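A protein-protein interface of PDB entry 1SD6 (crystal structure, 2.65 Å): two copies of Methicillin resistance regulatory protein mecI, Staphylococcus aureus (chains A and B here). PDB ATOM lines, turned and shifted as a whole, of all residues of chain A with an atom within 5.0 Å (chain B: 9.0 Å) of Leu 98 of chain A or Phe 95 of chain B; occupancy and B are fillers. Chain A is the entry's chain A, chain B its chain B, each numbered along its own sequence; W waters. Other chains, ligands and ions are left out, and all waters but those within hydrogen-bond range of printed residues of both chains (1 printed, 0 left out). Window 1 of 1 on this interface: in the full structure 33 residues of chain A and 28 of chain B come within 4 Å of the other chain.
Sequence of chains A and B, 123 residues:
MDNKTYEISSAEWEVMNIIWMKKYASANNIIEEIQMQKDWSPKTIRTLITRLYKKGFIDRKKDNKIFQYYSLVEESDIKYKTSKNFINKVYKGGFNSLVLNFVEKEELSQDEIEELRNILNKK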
ATOM      1  N   ILE A  87     -17.311 -11.215 -25.640  1.00  0.00           N
ATOM      2  CA  ILE A  87     -18.676 -11.709 -25.410  1.00  0.00           C
ATOM      3  C   ILE A  87     -19.706 -10.966 -26.238  1.00  0.00           C
ATOM      4  O   ILE A  87     -20.495 -11.596 -26.917  1.00  0.00           O
ATOM      5  CB  ILE A  87     -19.103 -11.579 -23.943  1.00  0.00           C
ATOM      6  CG1 ILE A  87     -18.219 -12.465 -23.059  1.00  0.00           C
ATOM      7  CG2 ILE A  87     -20.547 -11.976 -23.801  1.00  0.00           C
ATOM      8  CD1 ILE A  87     -18.109 -11.970 -21.616  1.00  0.00           C
ATOM      9  N   TYR A  91     -21.030 -14.314 -28.022  1.00  0.00           N
ATOM     10  CA  TYR A  91     -22.148 -14.801 -27.229  1.00  0.00           C
ATOM     11  C   TYR A  91     -23.211 -13.738 -26.983  1.00  0.00           C
ATOM     12  O   TYR A  91     -23.148 -13.005 -25.998  1.00  0.00           O
ATOM     13  CB  TYR A  91     -21.633 -15.349 -25.904  1.00  0.00           C
ATOM     14  CG  TYR A  91     -20.854 -16.613 -26.080  1.00  0.00           C
ATOM     15  CD1 TYR A  91     -21.495 -17.805 -26.406  1.00  0.00           C
ATOM     16  CD2 TYR A  91     -19.463 -16.617 -25.975  1.00  0.00           C
ATOM     17  CE1 TYR A  91     -20.771 -18.978 -26.627  1.00  0.00           C
ATOM     18  CE2 TYR A  91     -18.720 -17.789 -26.194  1.00  0.00           C
ATOM     19  CZ  TYR A  91     -19.383 -18.965 -26.521  1.00  0.00           C
ATOM     20  OH  TYR A  91     -18.670 -20.123 -26.733  1.00  0.00           O
ATOM     21  N   GLY A  94     -24.739 -13.206 -23.424  1.00  0.00           N
ATOM     22  CA  GLY A  94     -23.897 -12.806 -22.314  1.00  0.00           C
ATOM     23  C   GLY A  94     -22.939 -13.829 -21.750  1.00  0.00           C
ATOM     24  O   GLY A  94     -22.857 -14.976 -22.204  1.00  0.00           O
ATOM     25  N   PHE A  95     -22.215 -13.387 -20.730  1.00  0.00           N
ATOM     26  CA  PHE A  95     -21.228 -14.197 -20.036  1.00  0.00           C
ATOM     27  C   PHE A  95     -21.643 -15.636 -19.771  1.00  0.00           C
ATOM     28  O   PHE A  95     -20.849 -16.561 -19.921  1.00  0.00           O
ATOM     29  CB  PHE A  95     -20.880 -13.540 -18.708  1.00  0.00           C
ATOM     30  CG  PHE A  95     -19.892 -14.328 -17.887  1.00  0.00           C
ATOM     31  CD1 PHE A  95     -18.652 -14.698 -18.430  1.00  0.00           C
ATOM     32  CD2 PHE A  95     -20.154 -14.637 -16.551  1.00  0.00           C
ATOM     33  CE1 PHE A  95     -17.687 -15.361 -17.655  1.00  0.00           C
ATOM     34  CE2 PHE A  95     -19.200 -15.296 -15.780  1.00  0.00           C
ATOM     35  CZ  PHE A  95     -17.955 -15.653 -16.339  1.00  0.00           C
ATOM     36  N   ASN A  96     -22.884 -15.815 -19.351  1.00  0.00           N
ATOM     37  CA  ASN A  96     -23.405 -17.127 -19.039  1.00  0.00           C
ATOM     38  C   ASN A  96     -23.500 -18.038 -20.250  1.00  0.00           C
ATOM     39  O   ASN A  96     -23.353 -19.257 -20.126  1.00  0.00           O
ATOM     40  CB  ASN A  96     -24.765 -16.974 -18.392  1.00  0.00           C
ATOM     41  CG  ASN A  96     -24.759 -15.929 -17.316  1.00  0.00           C
ATOM     42  OD1 ASN A  96     -24.782 -14.726 -17.602  1.00  0.00           O
ATOM     43  ND2 ASN A  96     -24.706 -16.369 -16.065  1.00  0.00           N
ATOM     44  N   SER A  97     -23.757 -17.463 -21.415  1.00  0.00           N
ATOM     45  CA  SER A  97     -23.836 -18.264 -22.623  1.00  0.00           C
ATOM     46  C   SER A  97     -22.487 -18.956 -22.779  1.00  0.00           C
ATOM     47  O   SER A  97     -22.383 -20.159 -23.069  1.00  0.00           O
ATOM     48  CB  SER A  97     -24.092 -17.361 -23.825  1.00  0.00           C
ATOM     49  OG  SER A  97     -25.467 -17.244 -24.083  1.00  0.00           O
ATOM     50  N   LEU A  98     -21.454 -18.154 -22.565  1.00  0.00           N
ATOM     51  CA  LEU A  98     -20.076 -18.584 -22.669  1.00  0.00           C
ATOM     52  C   LEU A  98     -19.764 -19.744 -21.746  1.00  0.00           C
ATOM     53  O   LEU A  98     -19.243 -20.784 -22.168  1.00  0.00           O
ATOM     54  CB  LEU A  98     -19.163 -17.409 -22.340  1.00  0.00           C
ATOM     55  CG  LEU A  98     -17.651 -17.502 -22.543  1.00  0.00           C
ATOM     56  CD1 LEU A  98     -17.090 -16.183 -22.044  1.00  0.00           C
ATOM     57  CD2 LEU A  98     -17.014 -18.670 -21.784  1.00  0.00           C
ATOM     58  N   VAL A  99     -20.068 -19.551 -20.475  1.00  0.00           N
ATOM     59  CA  VAL A  99     -19.812 -20.566 -19.474  1.00  0.00           C
ATOM     60  C   VAL A  99     -20.638 -21.841 -19.739  1.00  0.00           C
ATOM     61  O   VAL A  99     -20.090 -22.961 -19.676  1.00  0.00           O
ATOM     62  CB  VAL A  99     -20.083 -19.999 -18.055  1.00  0.00           C
ATOM     63  CG1 VAL A  99     -19.448 -20.880 -17.042  1.00  0.00           C
ATOM     64  CG2 VAL A  99     -19.513 -18.581 -17.922  1.00  0.00           C
ATOM     65  N   LEU A 100     -21.934 -21.681 -20.043  1.00  0.00           N
ATOM     66  CA  LEU A 100     -22.803 -22.826 -20.344  1.00  0.00           C
ATOM     67  C   LEU A 100     -22.266 -23.627 -21.552  1.00  0.00           C
ATOM     68  O   LEU A 100     -22.362 -24.869 -21.613  1.00  0.00           O
ATOM     69  CB  LEU A 100     -24.232 -22.345 -20.643  1.00  0.00           C
ATOM     70  CG  LEU A 100     -25.158 -23.395 -21.288  1.00  0.00           C
ATOM     71  CD1 LEU A 100     -25.358 -24.577 -20.354  1.00  0.00           C
ATOM     72  CD2 LEU A 100     -26.490 -22.773 -21.625  1.00  0.00           C
ATOM     73  N   ASN A 101     -21.713 -22.896 -22.514  1.00  0.00           N
ATOM     74  CA  ASN A 101     -21.154 -23.488 -23.712  1.00  0.00           C
ATOM     75  C   ASN A 101     -19.816 -24.149 -23.404  1.00  0.00           C
ATOM     76  O   ASN A 101     -19.532 -25.258 -23.872  1.00  0.00           O
ATOM     77  CB  ASN A 101     -20.995 -22.403 -24.782  1.00  0.00           C
ATOM     78  CG  ASN A 101     -20.278 -22.897 -26.028  1.00  0.00           C
ATOM     79  OD1 ASN A 101     -19.061 -22.758 -26.151  1.00  0.00           O
ATOM     80  ND2 ASN A 101     -21.032 -23.481 -26.960  1.00  0.00           N
ATOM     81  N   PHE A 102     -18.999 -23.490 -22.595  1.00  0.00           N
ATOM     82  CA  PHE A 102     -17.705 -24.041 -22.284  1.00  0.00           C
ATOM     83  C   PHE A 102     -17.770 -25.311 -21.470  1.00  0.00           C
ATOM     84  O   PHE A 102     -16.937 -26.205 -21.643  1.00  0.00           O
ATOM     85  CB  PHE A 102     -16.839 -23.012 -21.573  1.00  0.00           C
ATOM     86  CG  PHE A 102     -15.390 -23.317 -21.660  1.00  0.00           C
ATOM     87  CD1 PHE A 102     -14.812 -24.239 -20.800  1.00  0.00           C
ATOM     88  CD2 PHE A 102     -14.619 -22.758 -22.670  1.00  0.00           C
ATOM     89  CE1 PHE A 102     -13.473 -24.612 -20.950  1.00  0.00           C
ATOM     90  CE2 PHE A 102     -13.289 -23.120 -22.832  1.00  0.00           C
ATOM     91  CZ  PHE A 102     -12.711 -24.052 -21.970  1.00  0.00           C
ATOM     92  N   VAL A 103     -18.773 -25.387 -20.595  1.00  0.00           N
ATOM     93  CA  VAL A 103     -19.017 -26.529 -19.705  1.00  0.00           C
ATOM     94  C   VAL A 103     -19.527 -27.821 -20.364  1.00  0.00           C
ATOM     95  O   VAL A 103     -19.036 -28.934 -20.072  1.00  0.00           O
ATOM     96  CB  VAL A 103     -20.015 -26.118 -18.633  1.00  0.00           C
ATOM     97  CG1 VAL A 103     -20.542 -27.317 -17.893  1.00  0.00           C
ATOM     98  CG2 VAL A 103     -19.350 -25.172 -17.691  1.00  0.00           C
ATOM     99  N   LEU A 116     -13.413 -24.227 -10.060  1.00  0.00           N
ATOM    100  CA  LEU A 116     -14.345 -23.184 -10.500  1.00  0.00           C
ATOM    101  C   LEU A 116     -15.387 -22.876  -9.465  1.00  0.00           C
ATOM    102  O   LEU A 116     -15.974 -21.807  -9.487  1.00  0.00           O
ATOM    103  CB  LEU A 116     -15.096 -23.608 -11.751  1.00  0.00           C
ATOM    104  CG  LEU A 116     -14.408 -23.541 -13.101  1.00  0.00           C
ATOM    105  CD1 LEU A 116     -15.396 -24.012 -14.142  1.00  0.00           C
ATOM    106  CD2 LEU A 116     -13.923 -22.117 -13.387  1.00  0.00           C
ATOM    107  N   SER B  76     -22.737 -24.582 -31.379  1.00  0.00           N
ATOM    108  CA  SER B  76     -22.168 -24.754 -30.036  1.00  0.00           C
ATOM    109  C   SER B  76     -20.733 -25.255 -30.163  1.00  0.00           C
ATOM    110  O   SER B  76     -19.920 -25.109 -29.262  1.00  0.00           O
ATOM    111  CB  SER B  76     -23.003 -25.749 -29.217  1.00  0.00           C
ATOM    112  OG  SER B  76     -22.957 -27.058 -29.776  1.00  0.00           O
ATOM    113  N   LYS B  79     -18.641 -21.907 -31.646  1.00  0.00           N
ATOM    114  CA  LYS B  79     -18.390 -20.874 -30.669  1.00  0.00           C
ATOM    115  C   LYS B  79     -17.406 -21.416 -29.622  1.00  0.00           C
ATOM    116  O   LYS B  79     -16.458 -20.727 -29.223  1.00  0.00           O
ATOM    117  CB  LYS B  79     -19.697 -20.419 -30.014  1.00  0.00           C
ATOM    118  CG  LYS B  79     -20.607 -19.550 -30.876  1.00  0.00           C
ATOM    119  CD  LYS B  79     -21.790 -19.075 -30.028  1.00  0.00           C
ATOM    120  CE  LYS B  79     -22.874 -18.317 -30.810  1.00  0.00           C
ATOM    121  NZ  LYS B  79     -23.987 -17.809 -29.910  1.00  0.00           N
ATOM    122  N   TYR B  80     -17.614 -22.652 -29.185  1.00  0.00           N
ATOM    123  CA  TYR B  80     -16.699 -23.249 -28.217  1.00  0.00           C
ATOM    124  C   TYR B  80     -15.278 -23.138 -28.716  1.00  0.00           C
ATOM    125  O   TYR B  80     -14.379 -22.732 -27.963  1.00  0.00           O
ATOM    126  CB  TYR B  80     -17.014 -24.723 -27.993  1.00  0.00           C
ATOM    127  CG  TYR B  80     -15.975 -25.501 -27.186  1.00  0.00           C
ATOM    128  CD1 TYR B  80     -15.530 -25.052 -25.936  1.00  0.00           C
ATOM    129  CD2 TYR B  80     -15.456 -26.708 -27.669  1.00  0.00           C
ATOM    130  CE1 TYR B  80     -14.590 -25.791 -25.195  1.00  0.00           C
ATOM    131  CE2 TYR B  80     -14.523 -27.449 -26.933  1.00  0.00           C
ATOM    132  CZ  TYR B  80     -14.096 -26.987 -25.705  1.00  0.00           C
ATOM    133  OH  TYR B  80     -13.175 -27.734 -25.001  1.00  0.00           O
ATOM    134  N   THR B  82     -14.049 -21.113 -30.873  1.00  0.00           N
ATOM    135  CA  THR B  82     -13.723 -19.692 -30.875  1.00  0.00           C
ATOM    136  C   THR B  82     -13.236 -19.250 -29.501  1.00  0.00           C
ATOM    137  O   THR B  82     -12.180 -18.629 -29.371  1.00  0.00           O
ATOM    138  CB  THR B  82     -14.975 -18.850 -31.230  1.00  0.00           C
ATOM    139  OG1 THR B  82     -15.332 -19.086 -32.594  1.00  0.00           O
ATOM    140  CG2 THR B  82     -14.738 -17.343 -31.009  1.00  0.00           C
ATOM    141  N   SER B  83     -14.029 -19.540 -28.476  1.00  0.00           N
ATOM    142  CA  SER B  83     -13.668 -19.201 -27.107  1.00  0.00           C
ATOM    143  C   SER B  83     -12.318 -19.796 -26.712  1.00  0.00           C
ATOM    144  O   SER B  83     -11.483 -19.108 -26.127  1.00  0.00           O
ATOM    145  CB  SER B  83     -14.722 -19.728 -26.163  1.00  0.00           C
ATOM    146  OG  SER B  83     -15.988 -19.311 -26.570  1.00  0.00           O
ATOM    147  N   LYS B  84     -12.125 -21.075 -27.019  1.00  0.00           N
ATOM    148  CA  LYS B  84     -10.880 -21.742 -26.702  1.00  0.00           C
ATOM    149  C   LYS B  84      -9.697 -21.014 -27.321  1.00  0.00           C
ATOM    150  O   LYS B  84      -8.619 -20.968 -26.745  1.00  0.00           O
ATOM    151  CB  LYS B  84     -10.927 -23.205 -27.146  1.00  0.00           C
ATOM    152  CG  LYS B  84     -11.763 -24.036 -26.194  1.00  0.00           C
ATOM    153  CD  LYS B  84     -11.046 -25.300 -25.675  1.00  0.00           C
ATOM    154  CE  LYS B  84      -9.865 -25.039 -24.712  1.00  0.00           C
ATOM    155  NZ  LYS B  84     -10.202 -24.354 -23.421  1.00  0.00           N
ATOM    156  N   PHE B  86      -9.788 -17.680 -28.160  1.00  0.00           N
ATOM    157  CA  PHE B  86      -9.745 -16.338 -27.611  1.00  0.00           C
ATOM    158  C   PHE B  86      -9.043 -16.388 -26.259  1.00  0.00           C
ATOM    159  O   PHE B  86      -8.347 -15.461 -25.846  1.00  0.00           O
ATOM    160  CB  PHE B  86     -11.155 -15.774 -27.418  1.00  0.00           C
ATOM    161  CG  PHE B  86     -11.157 -14.446 -26.709  1.00  0.00           C
ATOM    162  CD1 PHE B  86     -10.939 -13.255 -27.423  1.00  0.00           C
ATOM    163  CD2 PHE B  86     -11.300 -14.391 -25.301  1.00  0.00           C
ATOM    164  CE1 PHE B  86     -10.857 -12.014 -26.751  1.00  0.00           C
ATOM    165  CE2 PHE B  86     -11.220 -13.164 -24.611  1.00  0.00           C
ATOM    166  CZ  PHE B  86     -10.999 -11.973 -25.336  1.00  0.00           C
ATOM    167  N   ILE B  87      -9.268 -17.487 -25.566  1.00  0.00           N
ATOM    168  CA  ILE B  87      -8.675 -17.714 -24.261  1.00  0.00           C
ATOM    169  C   ILE B  87      -7.179 -17.961 -24.336  1.00  0.00           C
ATOM    170  O   ILE B  87      -6.432 -17.507 -23.487  1.00  0.00           O
ATOM    171  CB  ILE B  87      -9.344 -18.918 -23.594  1.00  0.00           C
ATOM    172  CG1 ILE B  87     -10.749 -18.515 -23.150  1.00  0.00           C
ATOM    173  CG2 ILE B  87      -8.499 -19.434 -22.466  1.00  0.00           C
ATOM    174  CD1 ILE B  87     -11.610 -19.675 -22.704  1.00  0.00           C
ATOM    175  N   ASN B  88      -6.740 -18.700 -25.344  1.00  0.00           N
ATOM    176  CA  ASN B  88      -5.325 -18.996 -25.480  1.00  0.00           C
ATOM    177  C   ASN B  88      -4.599 -17.724 -25.810  1.00  0.00           C
ATOM    178  O   ASN B  88      -3.518 -17.472 -25.263  1.00  0.00           O
ATOM    179  CB  ASN B  88      -5.094 -20.060 -26.552  1.00  0.00           C
ATOM    180  CG  ASN B  88      -5.659 -21.414 -26.143  1.00  0.00           C
ATOM    181  OD1 ASN B  88      -5.822 -22.302 -26.970  1.00  0.00           O
ATOM    182  ND2 ASN B  88      -5.964 -21.569 -24.845  1.00  0.00           N
ATOM    183  N   TYR B  91      -5.775 -15.278 -22.274  1.00  0.00           N
ATOM    184  CA  TYR B  91      -5.529 -15.923 -20.968  1.00  0.00           C
ATOM    185  C   TYR B  91      -4.561 -17.081 -20.895  1.00  0.00           C
ATOM    186  O   TYR B  91      -4.645 -18.058 -21.655  1.00  0.00           O
ATOM    187  CB  TYR B  91      -6.854 -16.382 -20.356  1.00  0.00           C
ATOM    188  CG  TYR B  91      -7.748 -15.237 -20.017  1.00  0.00           C
ATOM    189  CD1 TYR B  91      -7.442 -14.401 -18.948  1.00  0.00           C
ATOM    190  CD2 TYR B  91      -8.848 -14.912 -20.821  1.00  0.00           C
ATOM    191  CE1 TYR B  91      -8.210 -13.257 -18.690  1.00  0.00           C
ATOM    192  CE2 TYR B  91      -9.621 -13.760 -20.568  1.00  0.00           C
ATOM    193  CZ  TYR B  91      -9.289 -12.948 -19.500  1.00  0.00           C
ATOM    194  OH  TYR B  91     -10.019 -11.826 -19.229  1.00  0.00           O
ATOM    195  N   LYS B  92      -3.640 -16.968 -19.951  1.00  0.00           N
ATOM    196  CA  LYS B  92      -2.669 -18.025 -19.759  1.00  0.00           C
ATOM    197  C   LYS B  92      -2.914 -18.748 -18.424  1.00  0.00           C
ATOM    198  O   LYS B  92      -1.991 -19.054 -17.663  1.00  0.00           O
ATOM    199  CB  LYS B  92      -1.222 -17.498 -19.871  1.00  0.00           C
ATOM    200  CG  LYS B  92      -0.719 -17.128 -21.306  1.00  0.00           C
ATOM    201  CD  LYS B  92      -1.305 -17.951 -22.514  1.00  0.00           C
ATOM    202  CE  LYS B  92      -1.374 -19.492 -22.343  1.00  0.00           C
ATOM    203  NZ  LYS B  92      -2.585 -19.974 -21.562  1.00  0.00           N
ATOM    204  N   GLY B  93      -4.193 -19.007 -18.164  1.00  0.00           N
ATOM    205  CA  GLY B  93      -4.622 -19.730 -16.980  1.00  0.00           C
ATOM    206  C   GLY B  93      -5.825 -20.519 -17.474  1.00  0.00           C
ATOM    207  O   GLY B  93      -6.579 -21.129 -16.696  1.00  0.00           O
ATOM    208  N   GLY B  94      -5.983 -20.488 -18.801  1.00  0.00           N
ATOM    209  CA  GLY B  94      -7.087 -21.153 -19.449  1.00  0.00           C
ATOM    210  C   GLY B  94      -8.406 -20.482 -19.081  1.00  0.00           C
ATOM    211  O   GLY B  94      -8.460 -19.280 -18.776  1.00  0.00           O
ATOM    212  N   PHE B  95      -9.467 -21.287 -19.093  1.00  0.00           N
ATOM    213  CA  PHE B  95     -10.827 -20.852 -18.788  1.00  0.00           C
ATOM    214  C   PHE B  95     -11.012 -20.294 -17.401  1.00  0.00           C
ATOM    215  O   PHE B  95     -11.606 -19.227 -17.199  1.00  0.00           O
ATOM    216  CB  PHE B  95     -11.761 -22.037 -18.921  1.00  0.00           C
ATOM    217  CG  PHE B  95     -13.193 -21.708 -18.690  1.00  0.00           C
ATOM    218  CD1 PHE B  95     -13.792 -20.634 -19.355  1.00  0.00           C
ATOM    219  CD2 PHE B  95     -13.969 -22.507 -17.870  1.00  0.00           C
ATOM    220  CE1 PHE B  95     -15.146 -20.373 -19.205  1.00  0.00           C
ATOM    221  CE2 PHE B  95     -15.330 -22.249 -17.714  1.00  0.00           C
ATOM    222  CZ  PHE B  95     -15.919 -21.182 -18.385  1.00  0.00           C
ATOM    223  N   ASN B  96     -10.517 -21.061 -16.439  1.00  0.00           N
ATOM    224  CA  ASN B  96     -10.638 -20.723 -15.035  1.00  0.00           C
ATOM    225  C   ASN B  96     -10.182 -19.306 -14.727  1.00  0.00           C
ATOM    226  O   ASN B  96     -10.861 -18.572 -14.001  1.00  0.00           O
ATOM    227  CB  ASN B  96      -9.872 -21.762 -14.204  1.00  0.00           C
ATOM    228  CG  ASN B  96     -10.712 -23.039 -13.929  1.00  0.00           C
ATOM    229  OD1 ASN B  96     -11.631 -23.380 -14.685  1.00  0.00           O
ATOM    230  ND2 ASN B  96     -10.383 -23.748 -12.849  1.00  0.00           N
ATOM    231  N   SER B  97      -9.041 -18.943 -15.306  1.00  0.00           N
ATOM    232  CA  SER B  97      -8.413 -17.641 -15.158  1.00  0.00           C
ATOM    233  C   SER B  97      -9.260 -16.518 -15.773  1.00  0.00           C
ATOM    234  O   SER B  97      -9.269 -15.361 -15.289  1.00  0.00           O
ATOM    235  CB  SER B  97      -7.032 -17.697 -15.817  1.00  0.00           C
ATOM    236  OG  SER B  97      -6.374 -16.440 -15.827  1.00  0.00           O
ATOM    237  N   LEU B  98      -9.969 -16.856 -16.844  1.00  0.00           N
ATOM    238  CA  LEU B  98     -10.820 -15.883 -17.521  1.00  0.00           C
ATOM    239  C   LEU B  98     -11.981 -15.562 -16.636  1.00  0.00           C
ATOM    240  O   LEU B  98     -12.351 -14.403 -16.442  1.00  0.00           O
ATOM    241  CB  LEU B  98     -11.377 -16.456 -18.820  1.00  0.00           C
ATOM    242  CG  LEU B  98     -12.410 -15.593 -19.557  1.00  0.00           C
ATOM    243  CD1 LEU B  98     -12.487 -16.109 -20.958  1.00  0.00           C
ATOM    244  CD2 LEU B  98     -13.793 -15.606 -18.899  1.00  0.00           C
ATOM    245  N   VAL B  99     -12.571 -16.643 -16.151  1.00  0.00           N
ATOM    246  CA  VAL B  99     -13.735 -16.614 -15.280  1.00  0.00           C
ATOM    247  C   VAL B  99     -13.474 -15.832 -13.994  1.00  0.00           C
ATOM    248  O   VAL B  99     -14.320 -15.064 -13.541  1.00  0.00           O
ATOM    249  CB  VAL B  99     -14.153 -18.059 -14.957  1.00  0.00           C
ATOM    250  CG1 VAL B  99     -15.264 -18.074 -13.977  1.00  0.00           C
ATOM    251  CG2 VAL B  99     -14.575 -18.758 -16.241  1.00  0.00           C
ATOM    252  N   LEU B 100     -12.293 -16.045 -13.427  1.00  0.00           N
ATOM    253  CA  LEU B 100     -11.889 -15.377 -12.214  1.00  0.00           C
ATOM    254  C   LEU B 100     -11.831 -13.884 -12.437  1.00  0.00           C
ATOM    255  O   LEU B 100     -12.303 -13.099 -11.613  1.00  0.00           O
ATOM    256  CB  LEU B 100     -10.525 -15.879 -11.806  1.00  0.00           C
ATOM    257  CG  LEU B 100      -9.857 -15.206 -10.627  1.00  0.00           C
ATOM    258  CD1 LEU B 100     -10.843 -15.010  -9.497  1.00  0.00           C
ATOM    259  CD2 LEU B 100      -8.707 -16.087 -10.194  1.00  0.00           C
ATOM    260  N   ASN B 101     -11.245 -13.497 -13.563  1.00  0.00           N
ATOM    261  CA  ASN B 101     -11.115 -12.091 -13.919  1.00  0.00           C
ATOM    262  C   ASN B 101     -12.483 -11.448 -14.082  1.00  0.00           C
ATOM    263  O   ASN B 101     -12.715 -10.322 -13.649  1.00  0.00           O
ATOM    264  CB  ASN B 101     -10.324 -11.949 -15.224  1.00  0.00           C
ATOM    265  CG  ASN B 101     -10.291 -10.523 -15.728  1.00  0.00           C
ATOM    266  OD1 ASN B 101     -11.204 -10.079 -16.425  1.00  0.00           O
ATOM    267  ND2 ASN B 101      -9.249  -9.787 -15.354  1.00  0.00           N
ATOM    268  N   PHE B 102     -13.389 -12.180 -14.705  1.00  0.00           N
ATOM    269  CA  PHE B 102     -14.710 -11.661 -14.931  1.00  0.00           C
ATOM    270  C   PHE B 102     -15.472 -11.398 -13.637  1.00  0.00           C
ATOM    271  O   PHE B 102     -16.208 -10.416 -13.522  1.00  0.00           O
ATOM    272  CB  PHE B 102     -15.497 -12.623 -15.805  1.00  0.00           C
ATOM    273  CG  PHE B 102     -16.796 -12.057 -16.262  1.00  0.00           C
ATOM    274  CD1 PHE B 102     -17.895 -12.035 -15.410  1.00  0.00           C
ATOM    275  CD2 PHE B 102     -16.905 -11.470 -17.521  1.00  0.00           C
ATOM    276  CE1 PHE B 102     -19.083 -11.438 -15.804  1.00  0.00           C
ATOM    277  CE2 PHE B 102     -18.088 -10.866 -17.927  1.00  0.00           C
ATOM    278  CZ  PHE B 102     -19.177 -10.849 -17.069  1.00  0.00           C
ATOM    279  N   LEU B 116     -25.055 -18.745 -11.739  1.00  0.00           N
ATOM    280  CA  LEU B 116     -23.888 -19.445 -12.301  1.00  0.00           C
ATOM    281  C   LEU B 116     -23.616 -20.707 -11.510  1.00  0.00           C
ATOM    282  O   LEU B 116     -23.330 -21.758 -12.076  1.00  0.00           O
ATOM    283  CB  LEU B 116     -22.636 -18.576 -12.232  1.00  0.00           C
ATOM    284  CG  LEU B 116     -22.546 -17.342 -13.127  1.00  0.00           C
ATOM    285  CD1 LEU B 116     -21.242 -16.609 -12.877  1.00  0.00           C
ATOM    286  CD2 LEU B 116     -22.647 -17.758 -14.577  1.00  0.00           C
ATOM    287  N   ILE B 119     -25.366 -23.455 -13.238  1.00  0.00           N
ATOM    288  CA  ILE B 119     -24.847 -23.956 -14.513  1.00  0.00           C
ATOM    289  C   ILE B 119     -23.763 -24.997 -14.261  1.00  0.00           C
ATOM    290  O   ILE B 119     -23.763 -26.069 -14.867  1.00  0.00           O
ATOM    291  CB  ILE B 119     -24.233 -22.819 -15.343  1.00  0.00           C
ATOM    292  CG1 ILE B 119     -25.140 -21.585 -15.279  1.00  0.00           C
ATOM    293  CG2 ILE B 119     -24.048 -23.270 -16.771  1.00  0.00           C
ATOM    294  CD1 ILE B 119     -24.514 -20.322 -15.830  1.00  0.00           C
ATOM    295  N   LEU B 120     -22.860 -24.655 -13.344  1.00  0.00           N
ATOM    296  CA  LEU B 120     -21.723 -25.483 -12.931  1.00  0.00           C
ATOM    297  C   LEU B 120     -22.096 -26.860 -12.360  1.00  0.00           C
ATOM    298  O   LEU B 120     -21.416 -27.861 -12.633  1.00  0.00           O
ATOM    299  CB  LEU B 120     -20.909 -24.700 -11.887  1.00  0.00           C
ATOM    300  CG  LEU B 120     -19.412 -24.976 -11.716  1.00  0.00           C
ATOM    301  CD1 LEU B 120     -18.801 -23.981 -10.723  1.00  0.00           C
ATOM    302  CD2 LEU B 120     -19.210 -26.402 -11.255  1.00  0.00           C
HETATM  303  O   HOH W   1     -25.187 -16.965 -27.413  1.00  0.00           O
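Ile 87 of chain A touches Phe 102 of chain B, and with the chains exchanged Phe 102 of chain A touches Ile 87 of chain B. Phe 95 of chain A touches Phe 102 of chain B, and with the chains exchanged Phe 102 of chain A touches Phe 95 of chain B. Val 99 of chain A touches Phe 95 of chain B, but with the chains exchanged Phe 95 of chain A does not touch Val 99 of chain B (4.3 Å). Positions printed for both chains: 87, 91, 94, 95, 96, 97, 98, 99, 100, 101, 102 and 116. Of the 20 pairs that touch across the chains among the printed residues, 8 have their exchanged pair printed and touching as well.
Leu 98 of chain A touches just one residue of chain B: Phe 95. Of the printed residues of chain A, Lys 79 of chain B touches Tyr 91. Of the printed residues of chain A, Ser 83 of chain B touches Tyr 91 (2.8 Å). Of the printed residues of chain A, Leu 120 of chain B touches Leu 116. Printed residues of chain B within 4 Å of Asn 96 of chain A: Leu 116 (2.9 Å) and Ile 119 (3.96 Å). Gly 93 of chain B touches none of the printed residues of chain A. Ser 97 of chain B touches none of the printed residues of chain A. The nearest printed residue of chain A that does not touch Phe 95 of chain B is Val 103 of chain A (5.0 Å).
Water W1 bridges NZ of Lys 79 of chain B (2.9 Å) and OG of Ser 97 of chain A (3.4 Å).
OH of Tyr 91 of chain A sits at hydrogen-bond distance from OD1 of Asn 101 of chain A. The side-chain hydroxyl (OG) of Ser 83 of chain B lies within hydrogen-bond range of the backbone carbonyl oxygen (O) of Lys 79 of chain B. The backbone carbonyl oxygen (O) of Lys 84 of chain B sits close to the side-chain amide oxygen (OD1) of Asn 88 of chain B (3.1 Å).
Printed residues of chain B that touch a printed residue of chain A: Ser 76, Lys 79, Tyr 80, Ser 83, Lys 84, Ile 87, Phe 95, Asn 96, Phe 102, Leu 116, Ile 119 and Leu 120. Hydrophobic or aromatic side chains of chain A within 4 Å of the printed part of chain B: Ile 87, Tyr 91, Phe 95, Leu 98, Val 99, Leu 100, Phe 102 and Leu 116.
OH of Tyr 91 of chain A lies within hydrogen-bond range of O of Lys 79 of chain B (3.4 Å). The side-chain hydroxyl (OH) of Tyr 91 of chain A lies within hydrogen-bond range of the side-chain hydroxyl (OG) of Ser 83 of chain B (2.8 Å). ND2 of Asn 101 of chain A sits at hydrogen-bond distance from O of Ser 76 of chain B. The side-chain amide oxygen (OD1) of Asn 101 of chain A lies close to the backbone NH (N) of Tyr 80 of chain B, 3.4 Å away.
Phe 102 of chain B touches Phe 95 of chain A. Phe 95 of chain A touches Leu 116 of chain B. Asn 96 of chain A touches Leu 116 of chain B (ND2 to CD2, 2.9 Å). CD1 of Ile 119 of chain B touches ND2 of Asn 96 of chain A, 3.96 Å away. Phe 95 of chain B touches Leu 98 of chain A (CE1 to CD2, 3.6 Å). Phe 95 of chain B touches Val 99 of chain A (CZ to CG1, 3.8 Å). Ile 119 of chain B touches Leu 100 of chain A (CG2 to CA, 3.8 Å). CE2 of Phe 102 of chain A touches CE1 of Tyr 80 of chain B, at 3.8 Å. Phe 95 of chain B touches Phe 102 of chain A. Leu 116 of chain A touches Asn 96 of chain B (CD2 to OD1, 2.9 Å).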
